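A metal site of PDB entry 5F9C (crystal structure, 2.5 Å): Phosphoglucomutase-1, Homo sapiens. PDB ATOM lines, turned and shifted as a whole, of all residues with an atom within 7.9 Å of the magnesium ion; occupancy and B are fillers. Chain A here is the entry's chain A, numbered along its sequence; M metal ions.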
ATOM      1  N   SER A  20      22.200  32.732 -15.730  1.00  0.00           N
ATOM      2  CA  SER A  20      21.895  31.468 -16.374  1.00  0.00           C
ATOM      3  C   SER A  20      20.410  31.426 -16.764  1.00  0.00           C
ATOM      4  O   SER A  20      19.844  30.355 -17.025  1.00  0.00           O
ATOM      5  CB  SER A  20      22.241  30.312 -15.437  1.00  0.00           C
ATOM      6  OG  SER A  20      22.830  29.228 -16.136  1.00  0.00           O
ATOM      7  N   THR A  96      23.861  23.891 -25.228  1.00  0.00           N
ATOM      8  CA  THR A  96      24.188  25.307 -25.058  1.00  0.00           C
ATOM      9  C   THR A  96      25.413  25.727 -25.852  1.00  0.00           C
ATOM     10  O   THR A  96      25.405  26.788 -26.452  1.00  0.00           O
ATOM     11  CB  THR A  96      24.405  25.680 -23.556  1.00  0.00           C
ATOM     12  OG1 THR A  96      23.152  25.643 -22.882  1.00  0.00           O
ATOM     13  CG2 THR A  96      24.960  27.080 -23.411  1.00  0.00           C
ATOM     14  N   PRO A  97      26.473  24.897 -25.860  1.00  0.00           N
ATOM     15  CA  PRO A  97      27.543  25.274 -26.796  1.00  0.00           C
ATOM     16  C   PRO A  97      27.078  25.214 -28.288  1.00  0.00           C
ATOM     17  O   PRO A  97      27.570  25.977 -29.111  1.00  0.00           O
ATOM     18  CB  PRO A  97      28.633  24.242 -26.502  1.00  0.00           C
ATOM     19  CG  PRO A  97      28.367  23.788 -25.082  1.00  0.00           C
ATOM     20  CD  PRO A  97      26.854  23.770 -24.990  1.00  0.00           C
ATOM     21  N   THR A 115      16.902  25.432 -20.860  1.00  0.00           N
ATOM     22  CA  THR A 115      17.621  24.481 -20.019  1.00  0.00           C
ATOM     23  C   THR A 115      17.581  24.976 -18.607  1.00  0.00           C
ATOM     24  O   THR A 115      17.221  26.132 -18.347  1.00  0.00           O
ATOM     25  CB  THR A 115      19.100  24.318 -20.437  1.00  0.00           C
ATOM     26  OG1 THR A 115      19.740  23.356 -19.584  1.00  0.00           O
ATOM     27  CG2 THR A 115      19.847  25.644 -20.336  1.00  0.00           C
ATOM     28  N   ALA A 116      17.942  24.092 -17.684  1.00  0.00           N
ATOM     29  CA  ALA A 116      18.123  24.452 -16.288  1.00  0.00           C
ATOM     30  C   ALA A 116      19.354  23.745 -15.760  1.00  0.00           C
ATOM     31  O   ALA A 116      19.379  23.304 -14.604  1.00  0.00           O
ATOM     32  CB  ALA A 116      16.894  24.110 -15.475  1.00  0.00           C
ATOM     33  N   SER A 117      20.373  23.639 -16.624  1.00  0.00           N
ATOM     34  CA  SER A 117      21.721  23.188 -16.249  1.00  0.00           C
ATOM     35  C   SER A 117      21.695  21.812 -15.597  1.00  0.00           C
ATOM     36  O   SER A 117      21.281  20.824 -16.217  1.00  0.00           O
ATOM     37  CB  SER A 117      22.382  24.222 -15.307  1.00  0.00           C
ATOM     38  OG  SER A 117      23.782  24.355 -15.511  1.00  0.00           O
ATOM     39  N   HIS A 118      22.115  21.773 -14.337  1.00  0.00           N
ATOM     40  CA  HIS A 118      22.229  20.554 -13.550  1.00  0.00           C
ATOM     41  C   HIS A 118      20.934  20.174 -12.833  1.00  0.00           C
ATOM     42  O   HIS A 118      20.873  19.151 -12.144  1.00  0.00           O
ATOM     43  CB  HIS A 118      23.329  20.737 -12.497  1.00  0.00           C
ATOM     44  CG  HIS A 118      23.209  22.030 -11.747  1.00  0.00           C
ATOM     45  ND1 HIS A 118      23.621  23.238 -12.270  1.00  0.00           N
ATOM     46  CD2 HIS A 118      22.662  22.305 -10.539  1.00  0.00           C
ATOM     47  CE1 HIS A 118      23.354  24.200 -11.400  1.00  0.00           C
ATOM     48  NE2 HIS A 118      22.778  23.664 -10.344  1.00  0.00           N
ATOM     49  N   ASN A 119      19.915  21.006 -12.989  1.00  0.00           N
ATOM     50  CA  ASN A 119      18.716  20.866 -12.155  1.00  0.00           C
ATOM     51  C   ASN A 119      17.797  19.744 -12.665  1.00  0.00           C
ATOM     52  O   ASN A 119      17.721  19.503 -13.879  1.00  0.00           O
ATOM     53  CB  ASN A 119      17.967  22.207 -12.076  1.00  0.00           C
ATOM     54  CG  ASN A 119      18.781  23.265 -11.345  1.00  0.00           C
ATOM     55  OD1 ASN A 119      18.926  23.207 -10.125  1.00  0.00           O
ATOM     56  ND2 ASN A 119      19.311  24.228 -12.081  1.00  0.00           N
ATOM     57  N   PHE A 287      29.249  14.672 -18.581  1.00  0.00           N
ATOM     58  CA  PHE A 287      28.785  16.028 -18.866  1.00  0.00           C
ATOM     59  C   PHE A 287      27.586  16.376 -18.000  1.00  0.00           C
ATOM     60  O   PHE A 287      26.938  15.518 -17.417  1.00  0.00           O
ATOM     61  CB  PHE A 287      28.409  16.188 -20.353  1.00  0.00           C
ATOM     62  CG  PHE A 287      29.494  15.816 -21.313  1.00  0.00           C
ATOM     63  CD1 PHE A 287      30.678  16.552 -21.373  1.00  0.00           C
ATOM     64  CD2 PHE A 287      29.330  14.742 -22.200  1.00  0.00           C
ATOM     65  CE1 PHE A 287      31.689  16.225 -22.281  1.00  0.00           C
ATOM     66  CE2 PHE A 287      30.326  14.407 -23.093  1.00  0.00           C
ATOM     67  CZ  PHE A 287      31.508  15.138 -23.129  1.00  0.00           C
ATOM     68  N   ASP A 288      27.294  17.667 -17.895  1.00  0.00           N
ATOM     69  CA  ASP A 288      26.112  18.115 -17.184  1.00  0.00           C
ATOM     70  C   ASP A 288      24.918  18.224 -18.121  1.00  0.00           C
ATOM     71  O   ASP A 288      24.926  17.672 -19.233  1.00  0.00           O
ATOM     72  CB  ASP A 288      26.356  19.461 -16.526  1.00  0.00           C
ATOM     73  CG  ASP A 288      26.497  20.587 -17.542  1.00  0.00           C
ATOM     74  OD1 ASP A 288      27.072  20.336 -18.639  1.00  0.00           O
ATOM     75  OD2 ASP A 288      26.006  21.702 -17.259  1.00  0.00           O
ATOM     76  N   GLY A 289      23.903  18.927 -17.658  1.00  0.00           N
ATOM     77  CA  GLY A 289      22.613  18.967 -18.316  1.00  0.00           C
ATOM     78  C   GLY A 289      22.642  19.542 -19.717  1.00  0.00           C
ATOM     79  O   GLY A 289      22.087  18.956 -20.647  1.00  0.00           O
ATOM     80  N   ASP A 290      23.229  20.736 -19.839  1.00  0.00           N
ATOM     81  CA  ASP A 290      23.169  21.458 -21.102  1.00  0.00           C
ATOM     82  C   ASP A 290      24.487  21.489 -21.880  1.00  0.00           C
ATOM     83  O   ASP A 290      24.620  22.206 -22.877  1.00  0.00           O
ATOM     84  CB  ASP A 290      22.660  22.880 -20.849  1.00  0.00           C
ATOM     85  CG  ASP A 290      23.635  23.692 -20.065  1.00  0.00           C
ATOM     86  OD1 ASP A 290      24.450  23.090 -19.331  1.00  0.00           O
ATOM     87  OD2 ASP A 290      23.564  24.932 -20.188  1.00  0.00           O
ATOM     88  N   GLY A 291      25.486  20.734 -21.420  1.00  0.00           N
ATOM     89  CA  GLY A 291      26.732  20.545 -22.146  1.00  0.00           C
ATOM     90  C   GLY A 291      27.885  21.493 -21.930  1.00  0.00           C
ATOM     91  O   GLY A 291      28.913  21.393 -22.621  1.00  0.00           O
ATOM     92  N   ASP A 292      27.776  22.385 -20.943  1.00  0.00           N
ATOM     93  CA  ASP A 292      28.846  23.346 -20.748  1.00  0.00           C
ATOM     94  C   ASP A 292      29.841  22.944 -19.635  1.00  0.00           C
ATOM     95  O   ASP A 292      30.846  23.636 -19.410  1.00  0.00           O
ATOM     96  CB  ASP A 292      28.264  24.746 -20.489  1.00  0.00           C
ATOM     97  CG  ASP A 292      27.565  24.883 -19.149  1.00  0.00           C
ATOM     98  OD1 ASP A 292      27.251  23.864 -18.497  1.00  0.00           O
ATOM     99  OD2 ASP A 292      27.303  26.047 -18.766  1.00  0.00           O
ATOM    100  N   ARG A 293      29.601  21.797 -18.998  1.00  0.00           N
ATOM    101  CA  ARG A 293      30.543  21.289 -17.993  1.00  0.00           C
ATOM    102  C   ARG A 293      31.020  19.854 -18.298  1.00  0.00           C
ATOM    103  O   ARG A 293      30.337  19.077 -18.983  1.00  0.00           O
ATOM    104  CB  ARG A 293      29.907  21.349 -16.605  1.00  0.00           C
ATOM    105  CG  ARG A 293      29.608  22.756 -16.135  1.00  0.00           C
ATOM    106  CD  ARG A 293      28.897  22.768 -14.817  1.00  0.00           C
ATOM    107  NE  ARG A 293      28.289  24.065 -14.567  1.00  0.00           N
ATOM    108  CZ  ARG A 293      27.850  24.476 -13.381  1.00  0.00           C
ATOM    109  NH1 ARG A 293      27.986  23.696 -12.319  1.00  0.00           N
ATOM    110  NH2 ARG A 293      27.283  25.669 -13.269  1.00  0.00           N
ATOM    111  N   ASN A 294      32.197  19.513 -17.762  1.00  0.00           N
ATOM    112  CA  ASN A 294      32.813  18.223 -18.014  1.00  0.00           C
ATOM    113  C   ASN A 294      33.656  17.708 -16.836  1.00  0.00           C
ATOM    114  O   ASN A 294      34.369  18.484 -16.181  1.00  0.00           O
ATOM    115  CB  ASN A 294      33.693  18.304 -19.267  1.00  0.00           C
ATOM    116  CG  ASN A 294      34.984  19.071 -19.027  1.00  0.00           C
ATOM    117  OD1 ASN A 294      34.960  20.303 -18.936  1.00  0.00           O
ATOM    118  ND2 ASN A 294      36.105  18.358 -18.920  1.00  0.00           N
ATOM    119  N   SER A 378      34.740  24.509 -10.971  1.00  0.00           N
ATOM    120  CA  SER A 378      33.419  23.894 -11.083  1.00  0.00           C
ATOM    121  C   SER A 378      33.188  23.164 -12.447  1.00  0.00           C
ATOM    122  O   SER A 378      32.135  23.317 -13.067  1.00  0.00           O
ATOM    123  CB  SER A 378      32.331  24.945 -10.847  1.00  0.00           C
ATOM    124  OG  SER A 378      32.720  26.180 -11.417  1.00  0.00           O
ATOM    125  N   PHE A 379      34.169  22.385 -12.877  1.00  0.00           N
ATOM    126  CA  PHE A 379      34.013  21.480 -14.027  1.00  0.00           C
ATOM    127  C   PHE A 379      33.745  22.256 -15.314  1.00  0.00           C
ATOM    128  O   PHE A 379      32.963  21.824 -16.149  1.00  0.00           O
ATOM    129  CB  PHE A 379      32.884  20.477 -13.755  1.00  0.00           C
ATOM    130  CG  PHE A 379      33.198  19.535 -12.622  1.00  0.00           C
ATOM    131  CD1 PHE A 379      34.039  18.448 -12.811  1.00  0.00           C
ATOM    132  CD2 PHE A 379      32.657  19.745 -11.350  1.00  0.00           C
ATOM    133  CE1 PHE A 379      34.356  17.588 -11.757  1.00  0.00           C
ATOM    134  CE2 PHE A 379      32.952  18.879 -10.295  1.00  0.00           C
ATOM    135  CZ  PHE A 379      33.802  17.790 -10.505  1.00  0.00           C
ATOM    136  N   GLU A 388      30.375  30.321 -24.703  1.00  0.00           N
ATOM    137  CA  GLU A 388      29.854  29.538 -23.598  1.00  0.00           C
ATOM    138  C   GLU A 388      30.903  28.487 -23.320  1.00  0.00           C
ATOM    139  O   GLU A 388      31.785  28.233 -24.158  1.00  0.00           O
ATOM    140  CB  GLU A 388      28.496  28.901 -23.889  1.00  0.00           C
ATOM    141  CG  GLU A 388      27.319  29.874 -24.018  1.00  0.00           C
ATOM    142  CD  GLU A 388      26.724  30.281 -22.663  1.00  0.00           C
ATOM    143  OE1 GLU A 388      27.323  29.957 -21.606  1.00  0.00           O
ATOM    144  OE2 GLU A 388      25.634  30.914 -22.667  1.00  0.00           O
ATOM    145  N   LYS A 389      30.875  27.915 -22.119  1.00  0.00           N
ATOM    146  CA  LYS A 389      31.806  26.843 -21.805  1.00  0.00           C
ATOM    147  C   LYS A 389      31.381  25.612 -22.623  1.00  0.00           C
ATOM    148  O   LYS A 389      30.208  25.480 -22.967  1.00  0.00           O
ATOM    149  CB  LYS A 389      31.834  26.581 -20.301  1.00  0.00           C
ATOM    150  CG  LYS A 389      32.793  27.553 -19.579  1.00  0.00           C
ATOM    151  CD  LYS A 389      32.567  27.593 -18.071  1.00  0.00           C
ATOM    152  CE  LYS A 389      31.143  28.052 -17.729  1.00  0.00           C
ATOM    153  NZ  LYS A 389      30.217  26.909 -17.504  1.00  0.00           N
HETATM  154 MG    MG M   1      25.643  23.563 -17.438  1.00  0.00          MG
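The side-chain carboxylate (OD1) of Asp 288 sits at hydrogen-bond distance from the backbone NH (N) of Arg 293 (2.9 Å). The backbone NH (N) of Ser 117 is in hydrogen-bond range of the side-chain hydroxyl (OG1) of Thr 115, at 3.0 Å. The side-chain hydroxyl (OG1) of Thr 96 sits at hydrogen-bond distance from the side-chain carboxylate (OD2) of Asp 290, at 2.8 Å. The backbone NH (N) of Gly 291 sits at hydrogen-bond distance from the side-chain carboxylate (OD1) of Asp 288, at 3.2 Å. The side-chain carboxylate (OD2) of Asp 292 lies within salt-bridge range of the side-chain amino group (NZ) of Lys 389 (3.3 Å). OG of Ser 117 sits close to ND1 of His 118, 3.4 Å away.
Arg 293 touches the magnesium ion (NE to MG, 3.9 Å). Five residues have an atom within 4 Å of the magnesium ion: Ser 117, Asp 288, Asp 290, Asp 292 and Arg 293.
The magnesium ion is bound by OD2 of Asp 288 (1.9 Å), OD1 of Asp 292 (1.9 Å) and OD1 of Asp 290 (2.3 Å). Slightly farther from the magnesium ion lies the side-chain hydroxyl (OG) of Ser 117 (2.8 Å).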
